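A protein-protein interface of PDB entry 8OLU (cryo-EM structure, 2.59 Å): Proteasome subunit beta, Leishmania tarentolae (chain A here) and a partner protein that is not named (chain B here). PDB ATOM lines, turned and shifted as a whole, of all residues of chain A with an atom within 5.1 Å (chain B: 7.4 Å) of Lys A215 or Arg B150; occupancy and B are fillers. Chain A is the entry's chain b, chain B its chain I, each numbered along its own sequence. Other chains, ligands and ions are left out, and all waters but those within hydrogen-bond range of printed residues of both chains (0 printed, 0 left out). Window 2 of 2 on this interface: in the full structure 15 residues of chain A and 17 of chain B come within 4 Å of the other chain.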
ATOM      1  N   GLU A 209      -7.929  15.636  33.247  1.00  0.00           N
ATOM      2  CA  GLU A 209      -8.947  16.197  32.401  1.00  0.00           C
ATOM      3  C   GLU A 209      -8.824  15.578  31.004  1.00  0.00           C
ATOM      4  O   GLU A 209      -9.814  15.380  30.310  1.00  0.00           O
ATOM      5  CB  GLU A 209      -8.770  17.702  32.504  1.00  0.00           C
ATOM      6  CG  GLU A 209      -9.899  18.487  31.880  1.00  0.00           C
ATOM      7  CD  GLU A 209      -9.743  18.823  30.394  1.00  0.00           C
ATOM      8  OE1 GLU A 209      -8.767  19.591  30.056  1.00  0.00           O
ATOM      9  OE2 GLU A 209     -10.617  18.342  29.573  1.00  0.00           O
ATOM     10  N   GLY A 210      -7.621  15.134  30.648  1.00  0.00           N
ATOM     11  CA  GLY A 210      -7.374  14.602  29.331  1.00  0.00           C
ATOM     12  C   GLY A 210      -7.805  13.167  29.141  1.00  0.00           C
ATOM     13  O   GLY A 210      -7.580  12.602  28.088  1.00  0.00           O
ATOM     14  N   CYS A 212     -10.825  12.307  29.826  1.00  0.00           N
ATOM     15  CA  CYS A 212     -12.260  12.358  29.763  1.00  0.00           C
ATOM     16  C   CYS A 212     -12.723  11.782  28.431  1.00  0.00           C
ATOM     17  O   CYS A 212     -11.952  11.602  27.500  1.00  0.00           O
ATOM     18  CB  CYS A 212     -12.768  13.757  29.949  1.00  0.00           C
ATOM     19  SG  CYS A 212     -12.565  14.653  28.411  1.00  0.00           S
ATOM     20  N   PHE A 213     -13.976  11.381  28.399  1.00  0.00           N
ATOM     21  CA  PHE A 213     -14.540  10.703  27.265  1.00  0.00           C
ATOM     22  C   PHE A 213     -14.455  11.524  26.007  1.00  0.00           C
ATOM     23  O   PHE A 213     -14.260  10.995  24.940  1.00  0.00           O
ATOM     24  CB  PHE A 213     -16.011  10.462  27.581  1.00  0.00           C
ATOM     25  CG  PHE A 213     -16.635   9.384  26.753  1.00  0.00           C
ATOM     26  CD1 PHE A 213     -17.045   9.648  25.461  1.00  0.00           C
ATOM     27  CD2 PHE A 213     -16.691   8.082  27.243  1.00  0.00           C
ATOM     28  CE1 PHE A 213     -17.586   8.648  24.690  1.00  0.00           C
ATOM     29  CE2 PHE A 213     -17.235   7.080  26.446  1.00  0.00           C
ATOM     30  CZ  PHE A 213     -17.666   7.366  25.173  1.00  0.00           C
ATOM     31  N   GLU A 214     -14.731  12.814  26.118  1.00  0.00           N
ATOM     32  CA  GLU A 214     -14.776  13.676  24.958  1.00  0.00           C
ATOM     33  C   GLU A 214     -13.381  13.762  24.344  1.00  0.00           C
ATOM     34  O   GLU A 214     -13.229  13.653  23.132  1.00  0.00           O
ATOM     35  CB  GLU A 214     -15.347  15.020  25.364  1.00  0.00           C
ATOM     36  CG  GLU A 214     -15.558  15.927  24.156  1.00  0.00           C
ATOM     37  CD  GLU A 214     -16.156  17.320  24.398  1.00  0.00           C
ATOM     38  OE1 GLU A 214     -17.396  17.421  24.653  1.00  0.00           O
ATOM     39  OE2 GLU A 214     -15.386  18.316  24.318  1.00  0.00           O
ATOM     40  N   LYS A 215     -12.344  13.916  25.161  1.00  0.00           N
ATOM     41  CA  LYS A 215     -11.003  14.119  24.633  1.00  0.00           C
ATOM     42  C   LYS A 215     -10.414  12.852  24.024  1.00  0.00           C
ATOM     43  O   LYS A 215      -9.830  12.829  22.968  1.00  0.00           O
ATOM     44  CB  LYS A 215     -10.122  14.625  25.758  1.00  0.00           C
ATOM     45  CG  LYS A 215     -10.275  16.110  26.061  1.00  0.00           C
ATOM     46  CD  LYS A 215      -9.045  16.910  25.572  1.00  0.00           C
ATOM     47  CE  LYS A 215      -9.199  18.412  25.647  1.00  0.00           C
ATOM     48  NZ  LYS A 215      -9.397  18.841  27.053  1.00  0.00           N
ATOM     49  N   THR A 216     -10.641  11.739  24.648  1.00  0.00           N
ATOM     50  CA  THR A 216     -10.032  10.514  24.191  1.00  0.00           C
ATOM     51  C   THR A 216     -10.820   9.840  23.074  1.00  0.00           C
ATOM     52  O   THR A 216     -10.352   8.835  22.540  1.00  0.00           O
ATOM     53  CB  THR A 216      -9.917   9.607  25.405  1.00  0.00           C
ATOM     54  OG1 THR A 216     -11.226   9.444  25.924  1.00  0.00           O
ATOM     55  CG2 THR A 216      -9.055  10.229  26.463  1.00  0.00           C
ATOM     56  N   ALA A 217     -12.030  10.321  22.797  1.00  0.00           N
ATOM     57  CA  ALA A 217     -12.792   9.866  21.648  1.00  0.00           C
ATOM     58  C   ALA A 217     -12.010   9.974  20.349  1.00  0.00           C
ATOM     59  O   ALA A 217     -11.319  10.945  20.108  1.00  0.00           O
ATOM     60  CB  ALA A 217     -14.039  10.673  21.548  1.00  0.00           C
ATOM     61  N   ARG A 220     -15.212  12.645  16.449  1.00  0.00           N
ATOM     62  CA  ARG A 220     -15.985  13.776  16.957  1.00  0.00           C
ATOM     63  C   ARG A 220     -17.446  13.722  16.438  1.00  0.00           C
ATOM     64  O   ARG A 220     -18.375  14.050  17.237  1.00  0.00           O
ATOM     65  CB  ARG A 220     -15.323  15.094  16.533  1.00  0.00           C
ATOM     66  CG  ARG A 220     -13.851  15.253  16.898  1.00  0.00           C
ATOM     67  CD  ARG A 220     -13.631  15.737  18.326  1.00  0.00           C
ATOM     68  NE  ARG A 220     -12.221  16.012  18.636  1.00  0.00           N
ATOM     69  CZ  ARG A 220     -11.506  17.036  18.164  1.00  0.00           C
ATOM     70  NH1 ARG A 220     -10.214  17.138  18.444  1.00  0.00           N
ATOM     71  NH2 ARG A 220     -12.091  17.954  17.408  1.00  0.00           N
ATOM     72  OXT ARG A 220     -17.636  13.358  15.246  1.00  0.00           O
ATOM     73  N   VAL B  36       0.893  18.284  27.804  1.00  0.00           N
ATOM     74  CA  VAL B  36      -0.013  19.395  27.720  1.00  0.00           C
ATOM     75  C   VAL B  36       0.086  20.135  29.012  1.00  0.00           C
ATOM     76  O   VAL B  36       0.041  19.489  30.029  1.00  0.00           O
ATOM     77  CB  VAL B  36      -1.441  18.861  27.570  1.00  0.00           C
ATOM     78  CG1 VAL B  36      -2.447  19.967  27.631  1.00  0.00           C
ATOM     79  CG2 VAL B  36      -1.623  18.121  26.290  1.00  0.00           C
ATOM     80  N   LEU B 106      -5.633  18.210  14.450  1.00  0.00           N
ATOM     81  CA  LEU B 106      -6.304  16.983  14.133  1.00  0.00           C
ATOM     82  C   LEU B 106      -6.254  16.688  12.629  1.00  0.00           C
ATOM     83  O   LEU B 106      -6.298  15.517  12.285  1.00  0.00           O
ATOM     84  CB  LEU B 106      -7.724  17.085  14.683  1.00  0.00           C
ATOM     85  CG  LEU B 106      -8.662  15.968  14.215  1.00  0.00           C
ATOM     86  CD1 LEU B 106      -8.245  14.567  14.752  1.00  0.00           C
ATOM     87  CD2 LEU B 106     -10.068  16.285  14.616  1.00  0.00           C
ATOM     88  N   LEU B 109      -2.836  15.014  12.360  1.00  0.00           N
ATOM     89  CA  LEU B 109      -2.956  13.686  12.881  1.00  0.00           C
ATOM     90  C   LEU B 109      -3.686  12.808  11.903  1.00  0.00           C
ATOM     91  O   LEU B 109      -3.342  11.657  11.718  1.00  0.00           O
ATOM     92  CB  LEU B 109      -3.722  13.799  14.172  1.00  0.00           C
ATOM     93  CG  LEU B 109      -4.004  12.464  14.857  1.00  0.00           C
ATOM     94  CD1 LEU B 109      -2.925  12.193  15.897  1.00  0.00           C
ATOM     95  CD2 LEU B 109      -5.330  12.467  15.547  1.00  0.00           C
ATOM     96  N   GLY B 131       0.327  20.363  19.039  1.00  0.00           N
ATOM     97  CA  GLY B 131       0.133  21.708  18.611  1.00  0.00           C
ATOM     98  C   GLY B 131      -0.956  22.388  19.391  1.00  0.00           C
ATOM     99  O   GLY B 131      -1.491  21.843  20.311  1.00  0.00           O
ATOM    100  N   GLU B 135      -9.150  25.106  19.012  1.00  0.00           N
ATOM    101  CA  GLU B 135      -9.752  24.200  19.969  1.00  0.00           C
ATOM    102  C   GLU B 135      -8.878  23.905  21.198  1.00  0.00           C
ATOM    103  O   GLU B 135      -9.285  23.110  22.029  1.00  0.00           O
ATOM    104  CB  GLU B 135     -10.101  22.908  19.219  1.00  0.00           C
ATOM    105  CG  GLU B 135     -11.462  23.011  18.575  1.00  0.00           C
ATOM    106  CD  GLU B 135     -11.975  21.809  17.796  1.00  0.00           C
ATOM    107  OE1 GLU B 135     -11.281  20.760  17.788  1.00  0.00           O
ATOM    108  OE2 GLU B 135     -13.082  21.943  17.192  1.00  0.00           O
ATOM    109  N   GLY B 136      -7.655  24.440  21.254  1.00  0.00           N
ATOM    110  CA  GLY B 136      -6.762  24.328  22.404  1.00  0.00           C
ATOM    111  C   GLY B 136      -5.595  23.379  22.179  1.00  0.00           C
ATOM    112  O   GLY B 136      -5.293  22.955  21.066  1.00  0.00           O
ATOM    113  N   PRO B 137      -4.886  22.970  23.240  1.00  0.00           N
ATOM    114  CA  PRO B 137      -3.714  22.121  23.079  1.00  0.00           C
ATOM    115  C   PRO B 137      -4.124  20.738  22.632  1.00  0.00           C
ATOM    116  O   PRO B 137      -5.186  20.264  22.930  1.00  0.00           O
ATOM    117  CB  PRO B 137      -3.090  22.027  24.451  1.00  0.00           C
ATOM    118  CG  PRO B 137      -3.722  23.150  25.166  1.00  0.00           C
ATOM    119  CD  PRO B 137      -5.126  23.317  24.636  1.00  0.00           C
ATOM    120  N   PHE B 138      -3.217  20.119  21.917  1.00  0.00           N
ATOM    121  CA  PHE B 138      -3.541  18.860  21.354  1.00  0.00           C
ATOM    122  C   PHE B 138      -2.298  18.038  21.276  1.00  0.00           C
ATOM    123  O   PHE B 138      -1.461  18.275  20.454  1.00  0.00           O
ATOM    124  CB  PHE B 138      -4.067  19.030  19.954  1.00  0.00           C
ATOM    125  CG  PHE B 138      -4.646  17.779  19.368  1.00  0.00           C
ATOM    126  CD1 PHE B 138      -3.836  16.722  18.989  1.00  0.00           C
ATOM    127  CD2 PHE B 138      -6.000  17.659  19.214  1.00  0.00           C
ATOM    128  CE1 PHE B 138      -4.386  15.530  18.521  1.00  0.00           C
ATOM    129  CE2 PHE B 138      -6.548  16.526  18.655  1.00  0.00           C
ATOM    130  CZ  PHE B 138      -5.745  15.444  18.347  1.00  0.00           C
ATOM    131  N   LEU B 139      -2.239  16.998  22.047  1.00  0.00           N
ATOM    132  CA  LEU B 139      -1.062  16.194  21.997  1.00  0.00           C
ATOM    133  C   LEU B 139      -1.436  14.794  21.600  1.00  0.00           C
ATOM    134  O   LEU B 139      -2.353  14.265  22.161  1.00  0.00           O
ATOM    135  CB  LEU B 139      -0.472  16.270  23.379  1.00  0.00           C
ATOM    136  CG  LEU B 139       0.691  15.350  23.579  1.00  0.00           C
ATOM    137  CD1 LEU B 139       1.855  15.780  22.723  1.00  0.00           C
ATOM    138  CD2 LEU B 139       1.075  15.381  25.038  1.00  0.00           C
ATOM    139  N   ALA B 140      -0.690  14.159  20.723  1.00  0.00           N
ATOM    140  CA  ALA B 140      -1.115  12.822  20.381  1.00  0.00           C
ATOM    141  C   ALA B 140       0.039  11.938  20.005  1.00  0.00           C
ATOM    142  O   ALA B 140       1.053  12.459  19.632  1.00  0.00           O
ATOM    143  CB  ALA B 140      -2.085  12.889  19.266  1.00  0.00           C
ATOM    144  N   THR B 141      -0.131  10.643  20.146  1.00  0.00           N
ATOM    145  CA  THR B 141       0.815   9.749  19.547  1.00  0.00           C
ATOM    146  C   THR B 141       0.291   9.151  18.290  1.00  0.00           C
ATOM    147  O   THR B 141      -0.879   8.931  18.218  1.00  0.00           O
ATOM    148  CB  THR B 141       1.208   8.600  20.451  1.00  0.00           C
ATOM    149  OG1 THR B 141       0.185   8.032  21.282  1.00  0.00           O
ATOM    150  CG2 THR B 141       2.261   9.107  21.423  1.00  0.00           C
ATOM    151  N   THR B 148      -3.766   6.208  16.733  1.00  0.00           N
ATOM    152  CA  THR B 148      -3.519   7.359  17.553  1.00  0.00           C
ATOM    153  C   THR B 148      -4.119   7.231  18.927  1.00  0.00           C
ATOM    154  O   THR B 148      -5.085   6.507  19.142  1.00  0.00           O
ATOM    155  CB  THR B 148      -4.230   8.600  17.027  1.00  0.00           C
ATOM    156  OG1 THR B 148      -5.618   8.635  17.415  1.00  0.00           O
ATOM    157  CG2 THR B 148      -4.099   8.697  15.512  1.00  0.00           C
ATOM    158  N   ASP B 149      -3.592   8.064  19.806  1.00  0.00           N
ATOM    159  CA  ASP B 149      -3.992   8.130  21.192  1.00  0.00           C
ATOM    160  C   ASP B 149      -3.771   9.565  21.633  1.00  0.00           C
ATOM    161  O   ASP B 149      -2.689   9.931  21.983  1.00  0.00           O
ATOM    162  CB  ASP B 149      -3.155   7.221  22.104  1.00  0.00           C
ATOM    163  CG  ASP B 149      -3.369   5.677  22.077  1.00  0.00           C
ATOM    164  OD1 ASP B 149      -4.598   5.191  22.076  1.00  0.00           O
ATOM    165  OD2 ASP B 149      -2.299   4.901  22.181  1.00  0.00           O
ATOM    166  N   ARG B 150      -4.796  10.375  21.597  1.00  0.00           N
ATOM    167  CA  ARG B 150      -4.740  11.685  22.175  1.00  0.00           C
ATOM    168  C   ARG B 150      -4.707  11.623  23.672  1.00  0.00           C
ATOM    169  O   ARG B 150      -5.633  11.145  24.233  1.00  0.00           O
ATOM    170  CB  ARG B 150      -5.995  12.448  21.785  1.00  0.00           C
ATOM    171  CG  ARG B 150      -5.858  13.914  22.122  1.00  0.00           C
ATOM    172  CD  ARG B 150      -7.131  14.696  21.952  1.00  0.00           C
ATOM    173  NE  ARG B 150      -6.836  16.009  22.396  1.00  0.00           N
ATOM    174  CZ  ARG B 150      -7.642  17.005  22.200  1.00  0.00           C
ATOM    175  NH1 ARG B 150      -8.740  16.838  21.501  1.00  0.00           N
ATOM    176  NH2 ARG B 150      -7.381  18.158  22.754  1.00  0.00           N
ATOM    177  N   LEU B 151      -3.744  12.259  24.308  1.00  0.00           N
ATOM    178  CA  LEU B 151      -3.533  12.121  25.730  1.00  0.00           C
ATOM    179  C   LEU B 151      -2.838  13.331  26.258  1.00  0.00           C
ATOM    180  O   LEU B 151      -2.332  14.090  25.471  1.00  0.00           O
ATOM    181  CB  LEU B 151      -2.558  10.999  25.902  1.00  0.00           C
ATOM    182  CG  LEU B 151      -3.217   9.638  25.826  1.00  0.00           C
ATOM    183  CD1 LEU B 151      -2.197   8.528  25.981  1.00  0.00           C
ATOM    184  CD2 LEU B 151      -4.332   9.553  26.890  1.00  0.00           C
ATOM    185  N   PRO B 152      -2.855  13.581  27.553  1.00  0.00           N
ATOM    186  CA  PRO B 152      -2.161  14.691  28.116  1.00  0.00           C
ATOM    187  C   PRO B 152      -0.670  14.561  28.351  1.00  0.00           C
ATOM    188  O   PRO B 152      -0.040  15.516  28.709  1.00  0.00           O
ATOM    189  CB  PRO B 152      -2.744  14.860  29.499  1.00  0.00           C
ATOM    190  CG  PRO B 152      -3.486  13.649  29.785  1.00  0.00           C
ATOM    191  CD  PRO B 152      -3.667  12.888  28.511  1.00  0.00           C
ATOM    192  N   PHE B 153      -0.131  13.370  28.308  1.00  0.00           N
ATOM    193  CA  PHE B 153       1.285  13.241  28.278  1.00  0.00           C
ATOM    194  C   PHE B 153       1.580  11.998  27.510  1.00  0.00           C
ATOM    195  O   PHE B 153       0.780  11.121  27.530  1.00  0.00           O
ATOM    196  CB  PHE B 153       1.900  13.257  29.664  1.00  0.00           C
ATOM    197  CG  PHE B 153       1.285  12.350  30.672  1.00  0.00           C
ATOM    198  CD1 PHE B 153       0.124  12.721  31.325  1.00  0.00           C
ATOM    199  CD2 PHE B 153       1.825  11.094  30.907  1.00  0.00           C
ATOM    200  CE1 PHE B 153      -0.491  11.869  32.238  1.00  0.00           C
ATOM    201  CE2 PHE B 153       1.272  10.270  31.881  1.00  0.00           C
ATOM    202  CZ  PHE B 153       0.104  10.661  32.545  1.00  0.00           C
ATOM    203  N   VAL B 154       2.704  11.926  26.850  1.00  0.00           N
ATOM    204  CA  VAL B 154       2.998  10.777  26.054  1.00  0.00           C
ATOM    205  C   VAL B 154       4.476  10.610  25.955  1.00  0.00           C
ATOM    206  O   VAL B 154       5.207  11.525  26.235  1.00  0.00           O
ATOM    207  CB  VAL B 154       2.434  10.914  24.643  1.00  0.00           C
ATOM    208  CG1 VAL B 154       0.933  11.061  24.690  1.00  0.00           C
ATOM    209  CG2 VAL B 154       2.994  12.095  23.927  1.00  0.00           C
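Of the 18 printed residues of chain B, 5 touch a printed residue of chain A. Hydrophobic or aromatic side chains of chain B that line the printed part of chain A: Leu B106, Phe B138 and Pro B152. Among the printed residues, 6 pairs touch across the chains. Among the printed residues, Asp or Glu carboxylates within 4 Å of a Lys or Arg side-chain nitrogen of the other chain: Arg A220 with Glu B135.
The side-chain carboxylate (OE2) of Glu A209 lies within salt-bridge range of the side-chain amino group (NZ) of Lys A215, at 2.8 Å. The backbone NH (N) of Lys A215 sits at hydrogen-bond distance from the side-chain sulfur (SG) of Cys A212 (3.3 Å). N of Val B36 sits at hydrogen-bond distance from O of Pro B152, 3.1 Å away. The backbone NH of Phe B138 lies within hydrogen-bond range of the backbone carbonyl oxygen of Gly B131 (2.9 Å). O of Pro B137 sits at hydrogen-bond distance from NH2 of Arg B150 (3.0 Å).
The side-chain carboxylate of Glu B135 is in salt-bridge range of the guanidinium group of Arg A220 (2.9 Å). The guanidinium group (NH1) of Arg B150 sits close to the guanidinium group (NH1) of Arg A220 (3.4 Å).
Lys A215 touches just one residue of chain B: Arg B150. Arg B150 touches just these residues of chain A: Lys A215 (3.4 Å) and Arg A220 (3.4 Å). Of the printed residues of chain B, Arg A220 touches Leu B106, Glu B135, Phe B138 and Arg B150. Of the printed residues of chain A, Pro B152 touches Gly A210 (3.9 Å). Of the printed residues of chain A, Phe B138 touches Arg A220 (3.7 Å). Printed residues of chain B within 4 Å of Gly A210: Pro B152 (3.9 Å). Of the printed residues of chain A, Glu B135 touches Arg A220 (2.9 Å). The nearest residue of chain B that does not touch Lys A215 is Pro B137 (5.2 Å).
CD of Pro B152 touches O of Gly A210, 3.9 Å away. Arg B150 touches Lys A215 (NH2 to CE, 3.4 Å). Arg A220 touches Leu B106 (NH2 to CD2, 3.8 Å). Arg A220 touches Phe B138.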
